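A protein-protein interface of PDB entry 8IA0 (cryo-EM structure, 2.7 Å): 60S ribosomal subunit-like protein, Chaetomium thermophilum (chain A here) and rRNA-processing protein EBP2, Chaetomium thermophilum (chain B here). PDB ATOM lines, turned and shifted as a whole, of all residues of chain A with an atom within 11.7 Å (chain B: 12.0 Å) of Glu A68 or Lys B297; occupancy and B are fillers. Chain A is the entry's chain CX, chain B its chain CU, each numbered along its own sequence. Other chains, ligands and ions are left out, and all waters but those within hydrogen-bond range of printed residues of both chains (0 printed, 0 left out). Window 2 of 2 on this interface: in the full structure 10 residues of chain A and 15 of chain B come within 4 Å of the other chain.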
ATOM      1  N   VAL A  63     -10.714  18.509  14.874  1.00  0.00           N
ATOM      2  CA  VAL A  63     -11.042  18.037  13.537  1.00  0.00           C
ATOM      3  C   VAL A  63     -10.251  18.817  12.497  1.00  0.00           C
ATOM      4  O   VAL A  63     -10.425  20.026  12.349  1.00  0.00           O
ATOM      5  CB  VAL A  63     -12.551  18.143  13.263  1.00  0.00           C
ATOM      6  CG1 VAL A  63     -12.881  17.585  11.887  1.00  0.00           C
ATOM      7  CG2 VAL A  63     -13.339  17.417  14.343  1.00  0.00           C
ATOM      8  N   TYR A  64      -9.379  18.116  11.777  1.00  0.00           N
ATOM      9  CA  TYR A  64      -8.540  18.719  10.755  1.00  0.00           C
ATOM     10  C   TYR A  64      -8.637  17.908   9.472  1.00  0.00           C
ATOM     11  O   TYR A  64      -8.783  16.684   9.501  1.00  0.00           O
ATOM     12  CB  TYR A  64      -7.081  18.811  11.217  1.00  0.00           C
ATOM     13  CG  TYR A  64      -6.934  19.165  12.679  1.00  0.00           C
ATOM     14  CD1 TYR A  64      -7.371  20.393  13.163  1.00  0.00           C
ATOM     15  CD2 TYR A  64      -6.362  18.275  13.577  1.00  0.00           C
ATOM     16  CE1 TYR A  64      -7.241  20.722  14.498  1.00  0.00           C
ATOM     17  CE2 TYR A  64      -6.228  18.596  14.914  1.00  0.00           C
ATOM     18  CZ  TYR A  64      -6.669  19.821  15.370  1.00  0.00           C
ATOM     19  OH  TYR A  64      -6.537  20.145  16.700  1.00  0.00           O
ATOM     20  N   SER A  65      -8.555  18.607   8.344  1.00  0.00           N
ATOM     21  CA  SER A  65      -8.736  17.980   7.044  1.00  0.00           C
ATOM     22  C   SER A  65      -7.570  17.056   6.718  1.00  0.00           C
ATOM     23  O   SER A  65      -6.413  17.360   7.017  1.00  0.00           O
ATOM     24  CB  SER A  65      -8.873  19.044   5.956  1.00  0.00           C
ATOM     25  OG  SER A  65      -7.926  20.081   6.139  1.00  0.00           O
ATOM     26  N   GLU A  66      -7.887  15.916   6.099  1.00  0.00           N
ATOM     27  CA  GLU A  66      -6.845  15.006   5.640  1.00  0.00           C
ATOM     28  C   GLU A  66      -6.063  15.578   4.467  1.00  0.00           C
ATOM     29  O   GLU A  66      -4.963  15.096   4.178  1.00  0.00           O
ATOM     30  CB  GLU A  66      -7.450  13.656   5.255  1.00  0.00           C
ATOM     31  CG  GLU A  66      -8.535  13.169   6.202  1.00  0.00           C
ATOM     32  CD  GLU A  66      -9.319  12.000   5.637  1.00  0.00           C
ATOM     33  OE1 GLU A  66      -8.865  11.406   4.637  1.00  0.00           O
ATOM     34  OE2 GLU A  66     -10.387  11.675   6.196  1.00  0.00           O
ATOM     35  N   LYS A  67      -6.610  16.581   3.778  1.00  0.00           N
ATOM     36  CA  LYS A  67      -5.855  17.255   2.727  1.00  0.00           C
ATOM     37  C   LYS A  67      -4.730  18.095   3.315  1.00  0.00           C
ATOM     38  O   LYS A  67      -3.630  18.151   2.754  1.00  0.00           O
ATOM     39  CB  LYS A  67      -6.791  18.120   1.883  1.00  0.00           C
ATOM     40  CG  LYS A  67      -6.098  18.884   0.768  1.00  0.00           C
ATOM     41  CD  LYS A  67      -7.102  19.632  -0.093  1.00  0.00           C
ATOM     42  CE  LYS A  67      -7.695  20.816   0.655  1.00  0.00           C
ATOM     43  NZ  LYS A  67      -6.687  21.887   0.891  1.00  0.00           N
ATOM     44  N   GLU A  68      -4.991  18.759   4.443  1.00  0.00           N
ATOM     45  CA  GLU A  68      -3.967  19.581   5.079  1.00  0.00           C
ATOM     46  C   GLU A  68      -2.800  18.731   5.563  1.00  0.00           C
ATOM     47  O   GLU A  68      -1.634  19.115   5.407  1.00  0.00           O
ATOM     48  CB  GLU A  68      -4.586  20.374   6.231  1.00  0.00           C
ATOM     49  CG  GLU A  68      -3.696  20.544   7.448  1.00  0.00           C
ATOM     50  CD  GLU A  68      -4.165  21.667   8.352  1.00  0.00           C
ATOM     51  OE1 GLU A  68      -5.248  22.229   8.089  1.00  0.00           O
ATOM     52  OE2 GLU A  68      -3.448  21.989   9.323  1.00  0.00           O
ATOM     53  N   LEU A  69      -3.089  17.574   6.149  1.00  0.00           N
ATOM     54  CA  LEU A  69      -2.047  16.659   6.592  1.00  0.00           C
ATOM     55  C   LEU A  69      -1.495  15.877   5.407  1.00  0.00           C
ATOM     56  O   LEU A  69      -2.239  15.471   4.512  1.00  0.00           O
ATOM     57  CB  LEU A  69      -2.600  15.695   7.641  1.00  0.00           C
ATOM     58  CG  LEU A  69      -3.340  16.325   8.820  1.00  0.00           C
ATOM     59  CD1 LEU A  69      -4.057  15.262   9.629  1.00  0.00           C
ATOM     60  CD2 LEU A  69      -2.380  17.113   9.697  1.00  0.00           C
ATOM     61  N   GLY A  70      -0.182  15.666   5.406  1.00  0.00           N
ATOM     62  CA  GLY A  70       0.445  14.906   4.342  1.00  0.00           C
ATOM     63  C   GLY A  70       0.253  13.416   4.525  1.00  0.00           C
ATOM     64  O   GLY A  70       1.200  12.691   4.845  1.00  0.00           O
ATOM     65  N   ILE A  71      -0.974  12.949   4.326  1.00  0.00           N
ATOM     66  CA  ILE A  71      -1.358  11.580   4.649  1.00  0.00           C
ATOM     67  C   ILE A  71      -1.196  10.732   3.391  1.00  0.00           C
ATOM     68  O   ILE A  71      -1.754  11.092   2.343  1.00  0.00           O
ATOM     69  CB  ILE A  71      -2.794  11.520   5.178  1.00  0.00           C
ATOM     70  CG1 ILE A  71      -2.794  11.711   6.690  1.00  0.00           C
ATOM     71  CG2 ILE A  71      -3.439  10.189   4.839  1.00  0.00           C
ATOM     72  CD1 ILE A  71      -4.161  11.902   7.264  1.00  0.00           C
ATOM     73  N   PRO A  72      -0.439   9.636   3.439  1.00  0.00           N
ATOM     74  CA  PRO A  72      -0.275   8.800   2.245  1.00  0.00           C
ATOM     75  C   PRO A  72      -1.597   8.203   1.789  1.00  0.00           C
ATOM     76  O   PRO A  72      -2.470   7.875   2.594  1.00  0.00           O
ATOM     77  CB  PRO A  72       0.698   7.707   2.706  1.00  0.00           C
ATOM     78  CG  PRO A  72       1.369   8.268   3.914  1.00  0.00           C
ATOM     79  CD  PRO A  72       0.358   9.145   4.574  1.00  0.00           C
ATOM     80  N   GLN A  73      -1.734   8.065   0.474  1.00  0.00           N
ATOM     81  CA  GLN A  73      -2.918   7.451  -0.108  1.00  0.00           C
ATOM     82  C   GLN A  73      -2.814   5.932  -0.053  1.00  0.00           C
ATOM     83  O   GLN A  73      -1.747   5.358  -0.285  1.00  0.00           O
ATOM     84  CB  GLN A  73      -3.111   7.930  -1.544  1.00  0.00           C
ATOM     85  CG  GLN A  73      -2.610   9.342  -1.771  1.00  0.00           C
ATOM     86  CD  GLN A  73      -2.731   9.783  -3.210  1.00  0.00           C
ATOM     87  OE1 GLN A  73      -3.809  10.152  -3.671  1.00  0.00           O
ATOM     88  NE2 GLN A  73      -1.612   9.783  -3.921  1.00  0.00           N
ATOM     89  N   LYS A  86       3.718  15.289  -4.894  1.00  0.00           N
ATOM     90  CA  LYS A  86       3.239  16.470  -4.192  1.00  0.00           C
ATOM     91  C   LYS A  86       4.099  17.681  -4.529  1.00  0.00           C
ATOM     92  O   LYS A  86       5.314  17.568  -4.708  1.00  0.00           O
ATOM     93  CB  LYS A  86       3.238  16.231  -2.683  1.00  0.00           C
ATOM     94  CG  LYS A  86       2.601  17.348  -1.872  1.00  0.00           C
ATOM     95  CD  LYS A  86       1.085  17.244  -1.887  1.00  0.00           C
ATOM     96  CE  LYS A  86       0.573  16.456  -0.692  1.00  0.00           C
ATOM     97  NZ  LYS A  86       0.714  17.220   0.578  1.00  0.00           N
ATOM     98  N   GLY A  87       3.458  18.844  -4.615  1.00  0.00           N
ATOM     99  CA  GLY A  87       4.167  20.065  -4.928  1.00  0.00           C
ATOM    100  C   GLY A  87       4.627  20.179  -6.359  1.00  0.00           C
ATOM    101  O   GLY A  87       5.552  20.945  -6.642  1.00  0.00           O
ATOM    102  N   LYS B 286      -5.411   3.946   7.924  1.00  0.00           N
ATOM    103  CA  LYS B 286      -5.548   5.369   7.626  1.00  0.00           C
ATOM    104  C   LYS B 286      -5.819   6.175   8.889  1.00  0.00           C
ATOM    105  O   LYS B 286      -5.293   7.282   9.051  1.00  0.00           O
ATOM    106  CB  LYS B 286      -6.660   5.595   6.602  1.00  0.00           C
ATOM    107  CG  LYS B 286      -6.424   6.795   5.702  1.00  0.00           C
ATOM    108  CD  LYS B 286      -7.621   7.730   5.680  1.00  0.00           C
ATOM    109  CE  LYS B 286      -8.922   6.966   5.533  1.00  0.00           C
ATOM    110  NZ  LYS B 286     -10.050   7.861   5.157  1.00  0.00           N
ATOM    111  N   LYS B 288      -4.853   5.591  11.977  1.00  0.00           N
ATOM    112  CA  LYS B 288      -3.648   5.763  12.780  1.00  0.00           C
ATOM    113  C   LYS B 288      -2.733   6.820  12.175  1.00  0.00           C
ATOM    114  O   LYS B 288      -2.114   7.606  12.902  1.00  0.00           O
ATOM    115  CB  LYS B 288      -2.912   4.432  12.941  1.00  0.00           C
ATOM    116  CG  LYS B 288      -1.477   4.597  13.403  1.00  0.00           C
ATOM    117  CD  LYS B 288      -1.069   3.527  14.397  1.00  0.00           C
ATOM    118  CE  LYS B 288      -0.067   2.564  13.801  1.00  0.00           C
ATOM    119  NZ  LYS B 288       0.811   1.951  14.833  1.00  0.00           N
ATOM    120  N   LEU B 289      -2.641   6.861  10.843  1.00  0.00           N
ATOM    121  CA  LEU B 289      -1.869   7.913  10.191  1.00  0.00           C
ATOM    122  C   LEU B 289      -2.460   9.288  10.478  1.00  0.00           C
ATOM    123  O   LEU B 289      -1.725  10.271  10.615  1.00  0.00           O
ATOM    124  CB  LEU B 289      -1.798   7.661   8.686  1.00  0.00           C
ATOM    125  CG  LEU B 289      -0.814   6.585   8.229  1.00  0.00           C
ATOM    126  CD1 LEU B 289      -1.184   6.075   6.848  1.00  0.00           C
ATOM    127  CD2 LEU B 289       0.607   7.121   8.245  1.00  0.00           C
ATOM    128  N   ILE B 290      -3.790   9.377  10.559  1.00  0.00           N
ATOM    129  CA  ILE B 290      -4.427  10.632  10.951  1.00  0.00           C
ATOM    130  C   ILE B 290      -4.017  11.012  12.367  1.00  0.00           C
ATOM    131  O   ILE B 290      -3.692  12.171  12.646  1.00  0.00           O
ATOM    132  CB  ILE B 290      -5.957  10.519  10.823  1.00  0.00           C
ATOM    133  CG1 ILE B 290      -6.365  10.285   9.371  1.00  0.00           C
ATOM    134  CG2 ILE B 290      -6.631  11.768  11.366  1.00  0.00           C
ATOM    135  CD1 ILE B 290      -7.856  10.182   9.162  1.00  0.00           C
ATOM    136  N   GLU B 291      -4.025  10.039  13.281  1.00  0.00           N
ATOM    137  CA  GLU B 291      -3.734  10.326  14.681  1.00  0.00           C
ATOM    138  C   GLU B 291      -2.299  10.801  14.871  1.00  0.00           C
ATOM    139  O   GLU B 291      -2.043  11.725  15.650  1.00  0.00           O
ATOM    140  CB  GLU B 291      -4.005   9.087  15.530  1.00  0.00           C
ATOM    141  CG  GLU B 291      -5.455   8.939  15.946  1.00  0.00           C
ATOM    142  CD  GLU B 291      -5.635   7.975  17.099  1.00  0.00           C
ATOM    143  OE1 GLU B 291      -5.255   6.794  16.955  1.00  0.00           O
ATOM    144  OE2 GLU B 291      -6.157   8.401  18.149  1.00  0.00           O
ATOM    145  N   GLU B 292      -1.345  10.175  14.178  1.00  0.00           N
ATOM    146  CA  GLU B 292       0.046  10.602  14.287  1.00  0.00           C
ATOM    147  C   GLU B 292       0.232  12.011  13.743  1.00  0.00           C
ATOM    148  O   GLU B 292       0.944  12.830  14.335  1.00  0.00           O
ATOM    149  CB  GLU B 292       0.960   9.618  13.558  1.00  0.00           C
ATOM    150  CG  GLU B 292       1.184   8.312  14.295  1.00  0.00           C
ATOM    151  CD  GLU B 292       1.256   7.121  13.360  1.00  0.00           C
ATOM    152  OE1 GLU B 292       1.201   7.325  12.129  1.00  0.00           O
ATOM    153  OE2 GLU B 292       1.378   5.982  13.856  1.00  0.00           O
ATOM    154  N   ALA B 293      -0.395  12.310  12.603  1.00  0.00           N
ATOM    155  CA  ALA B 293      -0.295  13.650  12.037  1.00  0.00           C
ATOM    156  C   ALA B 293      -0.955  14.682  12.941  1.00  0.00           C
ATOM    157  O   ALA B 293      -0.441  15.794  13.107  1.00  0.00           O
ATOM    158  CB  ALA B 293      -0.918  13.677  10.643  1.00  0.00           C
ATOM    159  N   THR B 294      -2.103  14.335  13.528  1.00  0.00           N
ATOM    160  CA  THR B 294      -2.781  15.255  14.434  1.00  0.00           C
ATOM    161  C   THR B 294      -1.919  15.562  15.652  1.00  0.00           C
ATOM    162  O   THR B 294      -1.819  16.719  16.076  1.00  0.00           O
ATOM    163  CB  THR B 294      -4.127  14.671  14.861  1.00  0.00           C
ATOM    164  OG1 THR B 294      -4.997  14.592  13.725  1.00  0.00           O
ATOM    165  CG2 THR B 294      -4.776  15.537  15.927  1.00  0.00           C
ATOM    166  N   ALA B 295      -1.282  14.539  16.222  1.00  0.00           N
ATOM    167  CA  ALA B 295      -0.429  14.748  17.387  1.00  0.00           C
ATOM    168  C   ALA B 295       0.776  15.615  17.040  1.00  0.00           C
ATOM    169  O   ALA B 295       1.173  16.487  17.821  1.00  0.00           O
ATOM    170  CB  ALA B 295       0.018  13.403  17.956  1.00  0.00           C
ATOM    171  N   LYS B 296       1.376  15.383  15.871  1.00  0.00           N
ATOM    172  CA  LYS B 296       2.539  16.167  15.466  1.00  0.00           C
ATOM    173  C   LYS B 296       2.170  17.628  15.246  1.00  0.00           C
ATOM    174  O   LYS B 296       2.916  18.535  15.633  1.00  0.00           O
ATOM    175  CB  LYS B 296       3.159  15.574  14.202  1.00  0.00           C
ATOM    176  CG  LYS B 296       4.674  15.658  14.164  1.00  0.00           C
ATOM    177  CD  LYS B 296       5.316  14.611  15.063  1.00  0.00           C
ATOM    178  CE  LYS B 296       4.685  13.240  14.874  1.00  0.00           C
ATOM    179  NZ  LYS B 296       4.672  12.822  13.443  1.00  0.00           N
ATOM    180  N   LYS B 297       1.019  17.877  14.620  1.00  0.00           N
ATOM    181  CA  LYS B 297       0.625  19.252  14.341  1.00  0.00           C
ATOM    182  C   LYS B 297       0.111  19.951  15.592  1.00  0.00           C
ATOM    183  O   LYS B 297       0.335  21.155  15.763  1.00  0.00           O
ATOM    184  CB  LYS B 297      -0.426  19.285  13.233  1.00  0.00           C
ATOM    185  CG  LYS B 297      -0.901  20.680  12.880  1.00  0.00           C
ATOM    186  CD  LYS B 297      -2.091  20.647  11.948  1.00  0.00           C
ATOM    187  CE  LYS B 297      -3.392  20.814  12.706  1.00  0.00           C
ATOM    188  NZ  LYS B 297      -4.546  20.809  11.773  1.00  0.00           N
ATOM    189  N   ALA B 298      -0.571  19.220  16.477  1.00  0.00           N
ATOM    190  CA  ALA B 298      -1.035  19.819  17.724  1.00  0.00           C
ATOM    191  C   ALA B 298       0.135  20.218  18.613  1.00  0.00           C
ATOM    192  O   ALA B 298       0.048  21.202  19.356  1.00  0.00           O
ATOM    193  CB  ALA B 298      -1.964  18.856  18.459  1.00  0.00           C
ATOM    194  N   ALA B 299       1.232  19.460  18.559  1.00  0.00           N
ATOM    195  CA  ALA B 299       2.413  19.815  19.338  1.00  0.00           C
ATOM    196  C   ALA B 299       2.987  21.152  18.891  1.00  0.00           C
ATOM    197  O   ALA B 299       3.380  21.978  19.724  1.00  0.00           O
ATOM    198  CB  ALA B 299       3.466  18.714  19.226  1.00  0.00           C
ATOM    199  N   ALA B 300       3.050  21.383  17.578  1.00  0.00           N
ATOM    200  CA  ALA B 300       3.542  22.660  17.074  1.00  0.00           C
ATOM    201  C   ALA B 300       2.621  23.806  17.473  1.00  0.00           C
ATOM    202  O   ALA B 300       3.088  24.886  17.849  1.00  0.00           O
ATOM    203  CB  ALA B 300       3.697  22.599  15.556  1.00  0.00           C
ATOM    204  N   GLU B 301       1.306  23.591  17.391  1.00  0.00           N
ATOM    205  CA  GLU B 301       0.361  24.627  17.796  1.00  0.00           C
ATOM    206  C   GLU B 301       0.468  24.914  19.286  1.00  0.00           C
ATOM    207  O   GLU B 301       0.300  26.060  19.720  1.00  0.00           O
ATOM    208  CB  GLU B 301      -1.063  24.210  17.430  1.00  0.00           C
ATOM    209  CG  GLU B 301      -1.322  24.144  15.933  1.00  0.00           C
ATOM    210  CD  GLU B 301      -2.712  24.617  15.561  1.00  0.00           C
ATOM    211  OE1 GLU B 301      -3.189  25.602  16.165  1.00  0.00           O
ATOM    212  OE2 GLU B 301      -3.329  24.007  14.663  1.00  0.00           O
ATOM    213  N   ALA B 302       0.737  23.883  20.089  1.00  0.00           N
ATOM    214  CA  ALA B 302       0.937  24.090  21.518  1.00  0.00           C
ATOM    215  C   ALA B 302       2.157  24.963  21.783  1.00  0.00           C
ATOM    216  O   ALA B 302       2.113  25.865  22.628  1.00  0.00           O
ATOM    217  CB  ALA B 302       1.080  22.743  22.225  1.00  0.00           C
ATOM    218  N   ARG B 303       3.258  24.703  21.075  1.00  0.00           N
ATOM    219  CA  ARG B 303       4.455  25.521  21.235  1.00  0.00           C
ATOM    220  C   ARG B 303       4.221  26.945  20.752  1.00  0.00           C
ATOM    221  O   ARG B 303       4.668  27.908  21.388  1.00  0.00           O
ATOM    222  CB  ARG B 303       5.624  24.887  20.481  1.00  0.00           C
ATOM    223  CG  ARG B 303       6.978  25.474  20.823  1.00  0.00           C
ATOM    224  CD  ARG B 303       8.087  24.754  20.080  1.00  0.00           C
ATOM    225  NE  ARG B 303       8.126  23.333  20.403  1.00  0.00           N
ATOM    226  CZ  ARG B 303       7.872  22.361  19.537  1.00  0.00           C
ATOM    227  NH1 ARG B 303       7.556  22.621  18.279  1.00  0.00           N
ATOM    228  NH2 ARG B 303       7.939  21.096  19.943  1.00  0.00           N
ATOM    229  N   LYS B 304       3.524  27.099  19.625  1.00  0.00           N
ATOM    230  CA  LYS B 304       3.272  28.428  19.082  1.00  0.00           C
ATOM    231  C   LYS B 304       2.372  29.240  20.004  1.00  0.00           C
ATOM    232  O   LYS B 304       2.572  30.447  20.178  1.00  0.00           O
ATOM    233  CB  LYS B 304       2.662  28.306  17.684  1.00  0.00           C
ATOM    234  CG  LYS B 304       2.273  29.622  17.042  1.00  0.00           C
ATOM    235  CD  LYS B 304       1.295  29.397  15.903  1.00  0.00           C
ATOM    236  CE  LYS B 304       0.288  30.526  15.811  1.00  0.00           C
ATOM    237  NZ  LYS B 304       0.943  31.826  15.505  1.00  0.00           N
ATOM    238  N   GLN B 305       1.372  28.592  20.607  1.00  0.00           N
ATOM    239  CA  GLN B 305       0.503  29.288  21.552  1.00  0.00           C
ATOM    240  C   GLN B 305       1.257  29.673  22.817  1.00  0.00           C
ATOM    241  O   GLN B 305       0.953  30.697  23.440  1.00  0.00           O
ATOM    242  CB  GLN B 305      -0.703  28.416  21.892  1.00  0.00           C
ATOM    243  CG  GLN B 305      -1.842  28.511  20.895  1.00  0.00           C
ATOM    244  CD  GLN B 305      -2.713  29.728  21.123  1.00  0.00           C
ATOM    245  OE1 GLN B 305      -2.843  30.584  20.249  1.00  0.00           O
ATOM    246  NE2 GLN B 305      -3.315  29.811  22.304  1.00  0.00           N
ATOM    247  N   ARG B 306       2.236  28.860  23.218  1.00  0.00           N
ATOM    248  CA  ARG B 306       2.991  29.152  24.433  1.00  0.00           C
ATOM    249  C   ARG B 306       3.845  30.403  24.269  1.00  0.00           C
ATOM    250  O   ARG B 306       4.069  31.138  25.236  1.00  0.00           O
ATOM    251  CB  ARG B 306       3.855  27.953  24.811  1.00  0.00           C
ATOM    252  CG  ARG B 306       3.308  27.148  25.975  1.00  0.00           C
ATOM    253  CD  ARG B 306       4.241  26.016  26.343  1.00  0.00           C
ATOM    254  NE  ARG B 306       3.703  24.721  25.946  1.00  0.00           N
ATOM    255  CZ  ARG B 306       4.301  23.892  25.102  1.00  0.00           C
ATOM    256  NH1 ARG B 306       5.460  24.196  24.539  1.00  0.00           N
ATOM    257  NH2 ARG B 306       3.722  22.732  24.814  1.00  0.00           N
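The side-chain carboxylate (OE1) of Glu A66 lies within salt-bridge range of the side-chain amino group (NZ) of Lys B286 (3.8 Å). The side-chain amino group (NZ) of Lys B297 lies within salt-bridge range of the side-chain carboxylate (OE2) of Glu A68, 2.9 Å away.
The side-chain hydroxyl of Thr B294 sits at hydrogen-bond distance from the backbone carbonyl oxygen of Ile B290.
Among the printed residues, pairs that only touch across the chains: Tyr A64 with Lys B297 (3.0 Å), Ile A71 with Ile B290 (3.5 Å), Tyr A64 with Thr B294 (3.5 Å) and Leu A69 with Ala B293 (3.7 Å).
Of chain A, only Tyr A64 and Glu A68 come within 4 Å of Lys B297. Tyr A64 touches just these residues of chain B: Thr B294 and Lys B297. Ser A65 touches none of the printed residues of chain B. No residue of chain B comes within 4 Å of Lys A67. No residue of chain B comes within 4 Å of Gly A70. Of the printed residues of chain A, Ala B293 touches Leu A69. Thr B294 touches just one residue of chain A: Tyr A64. No residue of chain A comes within 4 Å of Ala B295. Ala B300 touches none of the printed residues of chain A. No residue of chain A comes within 4 Å of Glu B301. Printed residues of chain A within 4 Å of Ile B290: Ile A71 (3.5 Å). Printed residues of chain A within 4 Å of Lys B286: Glu A66 (3.8 Å). Gly A87 touches none of the printed residues of chain B. The nearest residue of chain A that does not touch Lys B297 is Leu A69 (4.2 Å). The nearest printed residue of chain B that does not touch Ile A71 is Leu B289 (4.3 Å).
Printed residues of chain B that touch a printed residue of chain A: Lys B286, Ile B290, Ala B293, Thr B294 and Lys B297. Hydrophobic or aromatic side chains of chain B within 4 Å of the printed part of chain A: Ile B290 and Ala B293. Printed residues of chain A that touch a printed residue of chain B: Tyr A64, Glu A66, Glu A68, Leu A69 and Ile A71.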
